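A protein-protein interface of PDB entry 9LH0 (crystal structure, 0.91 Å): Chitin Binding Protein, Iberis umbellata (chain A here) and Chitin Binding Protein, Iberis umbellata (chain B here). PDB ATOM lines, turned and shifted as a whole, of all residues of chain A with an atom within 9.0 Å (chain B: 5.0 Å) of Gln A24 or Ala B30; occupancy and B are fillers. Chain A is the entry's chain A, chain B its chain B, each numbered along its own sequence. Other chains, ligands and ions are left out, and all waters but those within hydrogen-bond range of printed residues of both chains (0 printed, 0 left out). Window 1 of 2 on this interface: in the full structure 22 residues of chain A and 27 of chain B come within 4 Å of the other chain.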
ATOM      1  N   PHE A  14       0.540  11.871   9.426  1.00  0.00           N
ATOM      2  CA  PHE A  14       0.927  12.275   8.079  1.00  0.00           C
ATOM      3  C   PHE A  14      -0.251  12.186   7.121  1.00  0.00           C
ATOM      4  O   PHE A  14      -0.528  13.129   6.372  1.00  0.00           O
ATOM      5  CB  PHE A  14       2.070  11.379   7.611  1.00  0.00           C
ATOM      6  CG  PHE A  14       2.623  11.721   6.251  1.00  0.00           C
ATOM      7  CD1 PHE A  14       3.235  12.940   6.010  1.00  0.00           C
ATOM      8  CD2 PHE A  14       2.557  10.797   5.222  1.00  0.00           C
ATOM      9  CE1 PHE A  14       3.772  13.227   4.763  1.00  0.00           C
ATOM     10  CE2 PHE A  14       3.079  11.083   3.974  1.00  0.00           C
ATOM     11  CZ  PHE A  14       3.693  12.297   3.746  1.00  0.00           C
ATOM     12  N   ALA A  17      -2.871  14.773   7.827  1.00  0.00           N
ATOM     13  CA  ALA A  17      -2.398  16.071   7.361  1.00  0.00           C
ATOM     14  C   ALA A  17      -2.250  16.130   5.846  1.00  0.00           C
ATOM     15  O   ALA A  17      -1.445  16.918   5.326  1.00  0.00           O
ATOM     16  CB  ALA A  17      -1.091  16.447   8.058  1.00  0.00           C
ATOM     17  N   HIS A  18      -3.010  15.302   5.129  1.00  0.00           N
ATOM     18  CA  HIS A  18      -3.012  15.282   3.666  1.00  0.00           C
ATOM     19  C   HIS A  18      -1.627  14.997   3.089  1.00  0.00           C
ATOM     20  O   HIS A  18      -1.268  15.508   2.022  1.00  0.00           O
ATOM     21  CB  HIS A  18      -3.620  16.556   3.069  1.00  0.00           C
ATOM     22  CG  HIS A  18      -5.037  16.812   3.488  1.00  0.00           C
ATOM     23  ND1 HIS A  18      -5.982  17.319   2.622  1.00  0.00           N
ATOM     24  CD2 HIS A  18      -5.666  16.657   4.679  1.00  0.00           C
ATOM     25  CE1 HIS A  18      -7.133  17.450   3.257  1.00  0.00           C
ATOM     26  NE2 HIS A  18      -6.968  17.056   4.506  1.00  0.00           N
ATOM     27  N   ARG A  19      -0.850  14.175   3.796  1.00  0.00           N
ATOM     28  CA  ARG A  19       0.509  13.845   3.387  1.00  0.00           C
ATOM     29  C   ARG A  19       1.348  15.100   3.185  1.00  0.00           C
ATOM     30  O   ARG A  19       2.281  15.126   2.382  1.00  0.00           O
ATOM     31  CB  ARG A  19       0.521  12.913   2.178  1.00  0.00           C
ATOM     32  CG  ARG A  19      -0.253  11.652   2.473  1.00  0.00           C
ATOM     33  CD  ARG A  19       0.134  10.500   1.593  1.00  0.00           C
ATOM     34  NE  ARG A  19      -0.615   9.309   1.967  1.00  0.00           N
ATOM     35  CZ  ARG A  19      -0.387   8.098   1.490  1.00  0.00           C
ATOM     36  NH1 ARG A  19       0.606   7.866   0.651  1.00  0.00           N
ATOM     37  NH2 ARG A  19      -1.174   7.094   1.869  1.00  0.00           N
ATOM     38  N   LEU A  20       1.033  16.142   3.950  1.00  0.00           N
ATOM     39  CA  LEU A  20       1.735  17.416   3.841  1.00  0.00           C
ATOM     40  C   LEU A  20       1.767  17.905   2.391  1.00  0.00           C
ATOM     41  O   LEU A  20       2.777  18.407   1.909  1.00  0.00           O
ATOM     42  CB  LEU A  20       3.140  17.350   4.454  1.00  0.00           C
ATOM     43  CG  LEU A  20       3.218  16.843   5.893  1.00  0.00           C
ATOM     44  CD1 LEU A  20       4.684  16.751   6.322  1.00  0.00           C
ATOM     45  CD2 LEU A  20       2.421  17.729   6.834  1.00  0.00           C
ATOM     46  N   SER A  21       0.636  17.766   1.695  1.00  0.00           N
ATOM     47  CA  SER A  21       0.551  18.060   0.263  1.00  0.00           C
ATOM     48  C   SER A  21       1.065  19.447  -0.092  1.00  0.00           C
ATOM     49  O   SER A  21       1.719  19.624  -1.130  1.00  0.00           O
ATOM     50  CB  SER A  21      -0.909  17.928  -0.195  1.00  0.00           C
ATOM     51  OG  SER A  21      -1.768  18.848   0.462  1.00  0.00           O
ATOM     52  N   ALA A  22       0.720  20.456   0.712  1.00  0.00           N
ATOM     53  CA  ALA A  22       1.179  21.807   0.405  1.00  0.00           C
ATOM     54  C   ALA A  22       2.683  21.934   0.617  1.00  0.00           C
ATOM     55  O   ALA A  22       3.368  22.652  -0.122  1.00  0.00           O
ATOM     56  CB  ALA A  22       0.430  22.837   1.248  1.00  0.00           C
ATOM     57  N   CYS A  23       3.210  21.254   1.639  1.00  0.00           N
ATOM     58  CA  CYS A  23       4.656  21.212   1.815  1.00  0.00           C
ATOM     59  C   CYS A  23       5.337  20.521   0.642  1.00  0.00           C
ATOM     60  O   CYS A  23       6.407  20.953   0.209  1.00  0.00           O
ATOM     61  CB  CYS A  23       5.037  20.508   3.117  1.00  0.00           C
ATOM     62  SG  CYS A  23       4.301  21.233   4.605  1.00  0.00           S
ATOM     63  N   GLN A  24       4.747  19.435   0.131  1.00  0.00           N
ATOM     64  CA  GLN A  24       5.321  18.774  -1.038  1.00  0.00           C
ATOM     65  C   GLN A  24       5.400  19.724  -2.227  1.00  0.00           C
ATOM     66  O   GLN A  24       6.422  19.784  -2.919  1.00  0.00           O
ATOM     67  CB  GLN A  24       4.533  17.509  -1.386  1.00  0.00           C
ATOM     68  CG  GLN A  24       4.667  16.401  -0.354  1.00  0.00           C
ATOM     69  CD  GLN A  24       4.213  15.046  -0.872  1.00  0.00           C
ATOM     70  OE1 GLN A  24       4.470  14.689  -2.017  1.00  0.00           O
ATOM     71  NE2 GLN A  24       3.557  14.277  -0.016  1.00  0.00           N
ATOM     72  N   LYS A  25       4.333  20.482  -2.474  1.00  0.00           N
ATOM     73  CA  LYS A  25       4.354  21.448  -3.568  1.00  0.00           C
ATOM     74  C   LYS A  25       5.406  22.523  -3.330  1.00  0.00           C
ATOM     75  O   LYS A  25       6.105  22.934  -4.260  1.00  0.00           O
ATOM     76  CB  LYS A  25       2.967  22.079  -3.743  1.00  0.00           C
ATOM     77  CG  LYS A  25       1.914  21.137  -4.283  1.00  0.00           C
ATOM     78  CD  LYS A  25       0.567  21.822  -4.399  1.00  0.00           C
ATOM     79  CE  LYS A  25      -0.480  20.861  -4.929  1.00  0.00           C
ATOM     80  NZ  LYS A  25      -0.038  20.241  -6.207  1.00  0.00           N
ATOM     81  N   TRP A  26       5.524  22.998  -2.091  1.00  0.00           N
ATOM     82  CA  TRP A  26       6.511  24.021  -1.754  1.00  0.00           C
ATOM     83  C   TRP A  26       7.935  23.507  -1.955  1.00  0.00           C
ATOM     84  O   TRP A  26       8.787  24.200  -2.530  1.00  0.00           O
ATOM     85  CB  TRP A  26       6.297  24.473  -0.304  1.00  0.00           C
ATOM     86  CG  TRP A  26       7.276  25.519   0.099  1.00  0.00           C
ATOM     87  CD1 TRP A  26       8.428  25.340   0.818  1.00  0.00           C
ATOM     88  CD2 TRP A  26       7.229  26.907  -0.241  1.00  0.00           C
ATOM     89  NE1 TRP A  26       9.093  26.531   0.955  1.00  0.00           N
ATOM     90  CE2 TRP A  26       8.375  27.509   0.314  1.00  0.00           C
ATOM     91  CE3 TRP A  26       6.325  27.705  -0.958  1.00  0.00           C
ATOM     92  CZ2 TRP A  26       8.647  28.865   0.173  1.00  0.00           C
ATOM     93  CZ3 TRP A  26       6.600  29.049  -1.100  1.00  0.00           C
ATOM     94  CH2 TRP A  26       7.748  29.620  -0.532  1.00  0.00           C
ATOM     95  N   ILE A  27       8.196  22.292  -1.451  1.00  0.00           N
ATOM     96  CA  ILE A  27       9.481  21.605  -1.604  1.00  0.00           C
ATOM     97  C   ILE A  27       9.846  21.491  -3.080  1.00  0.00           C
ATOM     98  O   ILE A  27      10.972  21.796  -3.496  1.00  0.00           O
ATOM     99  CB  ILE A  27       9.411  20.224  -0.911  1.00  0.00           C
ATOM    100  CG1 ILE A  27       9.424  20.371   0.617  1.00  0.00           C
ATOM    101  CG2 ILE A  27      10.543  19.315  -1.351  1.00  0.00           C
ATOM    102  CD1 ILE A  27       8.907  19.156   1.371  1.00  0.00           C
ATOM    103  N   HIS A  28       8.885  21.057  -3.894  1.00  0.00           N
ATOM    104  CA  HIS A  28       9.104  20.906  -5.329  1.00  0.00           C
ATOM    105  C   HIS A  28       9.481  22.244  -5.960  1.00  0.00           C
ATOM    106  O   HIS A  28      10.452  22.339  -6.721  1.00  0.00           O
ATOM    107  CB  HIS A  28       7.833  20.344  -5.963  1.00  0.00           C
ATOM    108  CG  HIS A  28       7.937  20.114  -7.437  1.00  0.00           C
ATOM    109  ND1 HIS A  28       6.831  20.020  -8.253  1.00  0.00           N
ATOM    110  CD2 HIS A  28       9.012  19.947  -8.242  1.00  0.00           C
ATOM    111  CE1 HIS A  28       7.221  19.814  -9.498  1.00  0.00           C
ATOM    112  NE2 HIS A  28       8.540  19.764  -9.518  1.00  0.00           N
ATOM    113  N   LYS A  29       8.727  23.295  -5.627  1.00  0.00           N
ATOM    114  CA  LYS A  29       8.981  24.634  -6.150  1.00  0.00           C
ATOM    115  C   LYS A  29      10.383  25.113  -5.794  1.00  0.00           C
ATOM    116  O   LYS A  29      11.094  25.660  -6.643  1.00  0.00           O
ATOM    117  CB  LYS A  29       7.921  25.587  -5.590  1.00  0.00           C
ATOM    118  CG  LYS A  29       8.261  27.066  -5.636  1.00  0.00           C
ATOM    119  CD  LYS A  29       7.179  27.874  -4.927  1.00  0.00           C
ATOM    120  CE  LYS A  29       7.539  29.346  -4.839  1.00  0.00           C
ATOM    121  NZ  LYS A  29       7.787  29.933  -6.184  1.00  0.00           N
ATOM    122  N   GLN A  30      10.804  24.909  -4.546  1.00  0.00           N
ATOM    123  CA  GLN A  30      12.149  25.321  -4.155  1.00  0.00           C
ATOM    124  C   GLN A  30      13.213  24.493  -4.863  1.00  0.00           C
ATOM    125  O   GLN A  30      14.247  25.029  -5.275  1.00  0.00           O
ATOM    126  CB  GLN A  30      12.317  25.224  -2.639  1.00  0.00           C
ATOM    127  CG  GLN A  30      11.554  26.284  -1.872  1.00  0.00           C
ATOM    128  CD  GLN A  30      12.059  27.683  -2.161  1.00  0.00           C
ATOM    129  OE1 GLN A  30      13.215  27.879  -2.530  1.00  0.00           O
ATOM    130  NE2 GLN A  30      11.190  28.664  -2.001  1.00  0.00           N
ATOM    131  N   ALA A  31      12.974  23.189  -5.012  1.00  0.00           N
ATOM    132  CA  ALA A  31      13.982  22.302  -5.580  1.00  0.00           C
ATOM    133  C   ALA A  31      14.336  22.709  -7.003  1.00  0.00           C
ATOM    134  O   ALA A  31      15.516  22.747  -7.371  1.00  0.00           O
ATOM    135  CB  ALA A  31      13.500  20.856  -5.551  1.00  0.00           C
ATOM    136  N   THR B  26       8.110  12.895   9.094  1.00  0.00           N
ATOM    137  CA  THR B  26       7.108  13.046   8.046  1.00  0.00           C
ATOM    138  C   THR B  26       7.589  13.950   6.920  1.00  0.00           C
ATOM    139  O   THR B  26       7.217  13.735   5.762  1.00  0.00           O
ATOM    140  CB  THR B  26       5.778  13.550   8.615  1.00  0.00           C
ATOM    141  OG1 THR B  26       5.958  14.838   9.213  1.00  0.00           O
ATOM    142  CG2 THR B  26       5.214  12.563   9.641  1.00  0.00           C
ATOM    143  N   LEU B  27       8.414  14.952   7.225  1.00  0.00           N
ATOM    144  CA  LEU B  27       8.967  15.786   6.164  1.00  0.00           C
ATOM    145  C   LEU B  27       9.953  15.014   5.299  1.00  0.00           C
ATOM    146  O   LEU B  27      10.032  15.254   4.091  1.00  0.00           O
ATOM    147  CB  LEU B  27       9.608  17.038   6.756  1.00  0.00           C
ATOM    148  CG  LEU B  27       8.595  18.143   7.080  1.00  0.00           C
ATOM    149  CD1 LEU B  27       9.224  19.191   7.971  1.00  0.00           C
ATOM    150  CD2 LEU B  27       8.048  18.777   5.809  1.00  0.00           C
ATOM    151  N   ARG B  28      10.705  14.086   5.897  1.00  0.00           N
ATOM    152  CA  ARG B  28      11.570  13.212   5.109  1.00  0.00           C
ATOM    153  C   ARG B  28      10.744  12.343   4.170  1.00  0.00           C
ATOM    154  O   ARG B  28      11.088  12.177   2.995  1.00  0.00           O
ATOM    155  CB  ARG B  28      12.419  12.357   6.055  1.00  0.00           C
ATOM    156  CG  ARG B  28      13.121  11.174   5.426  1.00  0.00           C
ATOM    157  CD  ARG B  28      14.448  11.567   4.885  1.00  0.00           C
ATOM    158  NE  ARG B  28      15.210  10.390   4.504  1.00  0.00           N
ATOM    159  CZ  ARG B  28      16.410  10.441   3.953  1.00  0.00           C
ATOM    160  NH1 ARG B  28      17.000  11.598   3.700  1.00  0.00           N
ATOM    161  NH2 ARG B  28      17.032   9.307   3.651  1.00  0.00           N
ATOM    162  N   ARG B  29       9.631  11.798   4.672  1.00  0.00           N
ATOM    163  CA  ARG B  29       8.731  11.023   3.826  1.00  0.00           C
ATOM    164  C   ARG B  29       8.163  11.878   2.699  1.00  0.00           C
ATOM    165  O   ARG B  29       8.091  11.439   1.544  1.00  0.00           O
ATOM    166  CB  ARG B  29       7.604  10.442   4.685  1.00  0.00           C
ATOM    167  CG  ARG B  29       6.618   9.585   3.924  1.00  0.00           C
ATOM    168  CD  ARG B  29       5.634   8.907   4.856  1.00  0.00           C
ATOM    169  NE  ARG B  29       4.586   8.232   4.104  1.00  0.00           N
ATOM    170  CZ  ARG B  29       3.545   7.626   4.656  1.00  0.00           C
ATOM    171  NH1 ARG B  29       3.400   7.566   5.970  1.00  0.00           N
ATOM    172  NH2 ARG B  29       2.624   7.075   3.872  1.00  0.00           N
ATOM    173  N   ALA B  30       7.769  13.112   3.016  1.00  0.00           N
ATOM    174  CA  ALA B  30       7.234  14.016   2.001  1.00  0.00           C
ATOM    175  C   ALA B  30       8.280  14.340   0.940  1.00  0.00           C
ATOM    176  O   ALA B  30       7.966  14.408  -0.256  1.00  0.00           O
ATOM    177  CB  ALA B  30       6.744  15.300   2.672  1.00  0.00           C
ATOM    178  N   ALA B  31       9.528  14.555   1.365  1.00  0.00           N
ATOM    179  CA  ALA B  31      10.599  14.849   0.419  1.00  0.00           C
ATOM    180  C   ALA B  31      10.859  13.668  -0.506  1.00  0.00           C
ATOM    181  O   ALA B  31      11.019  13.844  -1.721  1.00  0.00           O
ATOM    182  CB  ALA B  31      11.872  15.239   1.172  1.00  0.00           C
ATOM    183  N   MET B  32      10.913  12.457   0.054  1.00  0.00           N
ATOM    184  CA  MET B  32      11.100  11.277  -0.781  1.00  0.00           C
ATOM    185  C   MET B  32       9.966  11.128  -1.781  1.00  0.00           C
ATOM    186  O   MET B  32      10.196  10.755  -2.933  1.00  0.00           O
ATOM    187  CB  MET B  32      11.203  10.018   0.075  1.00  0.00           C
ATOM    188  CG  MET B  32      12.477   9.874   0.875  1.00  0.00           C
ATOM    189  SD  MET B  32      12.390   8.346   1.831  1.00  0.00           S
ATOM    190  CE  MET B  32      13.642   7.347   1.037  1.00  0.00           C
ATOM    191  N   ALA B  33       8.735  11.417  -1.353  1.00  0.00           N
ATOM    192  CA  ALA B  33       7.579  11.303  -2.235  1.00  0.00           C
ATOM    193  C   ALA B  33       7.683  12.265  -3.414  1.00  0.00           C
ATOM    194  O   ALA B  33       7.477  11.869  -4.568  1.00  0.00           O
ATOM    195  CB  ALA B  33       6.293  11.540  -1.436  1.00  0.00           C
ATOM    196  N   VAL B  34       8.025  13.534  -3.141  1.00  0.00           N
ATOM    197  CA  VAL B  34       8.221  14.533  -4.201  1.00  0.00           C
ATOM    198  C   VAL B  34       9.329  14.108  -5.139  1.00  0.00           C
ATOM    199  O   VAL B  34       9.193  14.182  -6.367  1.00  0.00           O
ATOM    200  CB  VAL B  34       8.565  15.910  -3.600  1.00  0.00           C
ATOM    201  CG1 VAL B  34       9.020  16.886  -4.705  1.00  0.00           C
ATOM    202  CG2 VAL B  34       7.403  16.461  -2.861  1.00  0.00           C
ATOM    203  N   ARG B  37       8.052  11.036  -7.225  1.00  0.00           N
ATOM    204  CA  ARG B  37       6.889  11.298  -8.063  1.00  0.00           C
ATOM    205  C   ARG B  37       7.221  12.274  -9.185  1.00  0.00           C
ATOM    206  O   ARG B  37       6.742  12.117 -10.314  1.00  0.00           O
ATOM    207  CB  ARG B  37       5.751  11.826  -7.193  1.00  0.00           C
ATOM    208  CG  ARG B  37       4.379  11.511  -7.710  1.00  0.00           C
ATOM    209  CD  ARG B  37       3.322  11.806  -6.676  1.00  0.00           C
ATOM    210  NE  ARG B  37       3.375  13.195  -6.243  1.00  0.00           N
ATOM    211  CZ  ARG B  37       3.682  13.593  -5.016  1.00  0.00           C
ATOM    212  NH1 ARG B  37       3.856  12.728  -4.030  1.00  0.00           N
ATOM    213  NH2 ARG B  37       3.822  14.892  -4.775  1.00  0.00           N
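The guanidinium group of Arg B37 lies within hydrogen-bond range of the side-chain amide oxygen of Gln A24, 2.8 Å away.
The backbone NH (N) of Arg A19 lies within hydrogen-bond range of the backbone carbonyl oxygen (O) of Phe A14, at 2.8 Å.
O of Arg A19 lies within hydrogen-bond range of NE2 of Gln A24, 2.8 Å away.
Among the printed residues, pairs that only touch across the chains: Phe A14 with Thr B26 (3.6 Å), Phe A14 with Arg B29 (3.2 Å), Arg A19 with Arg B29 (3.9 Å), Leu A20 with Thr B26 (3.7 Å), Leu A20 with Leu B27 (3.96 Å), Gln A24 with Ala B30 (3.8 Å), Gln A24 with Ala B33 (3.7 Å), Gln A24 with Val B34 (3.4 Å) and His A28 with Val B34 (3.9 Å).
Of chain A, only Gln A24 (3.7 Å) comes within 4 Å of Ala B33.
Printed residues of chain B within 4 Å of His A28: Val B34 (3.9 Å).
Printed residues of chain A within 4 Å of Leu B27: Leu A20.
The nearest printed residue of chain B that does not touch Gln A24 is Ala B31 (5.5 Å).
The nearest printed residue of chain A that does not touch Arg B37 is Lys A25 (6.1 Å).
Hydrophobic or aromatic side chains of chain A within 4 Å of the printed part of chain B: Phe A14, Leu A20 and His A28.
Among the printed residues, no Asp or Glu carboxylate lies within 4 Å of a Lys or Arg side-chain nitrogen of the other chain.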
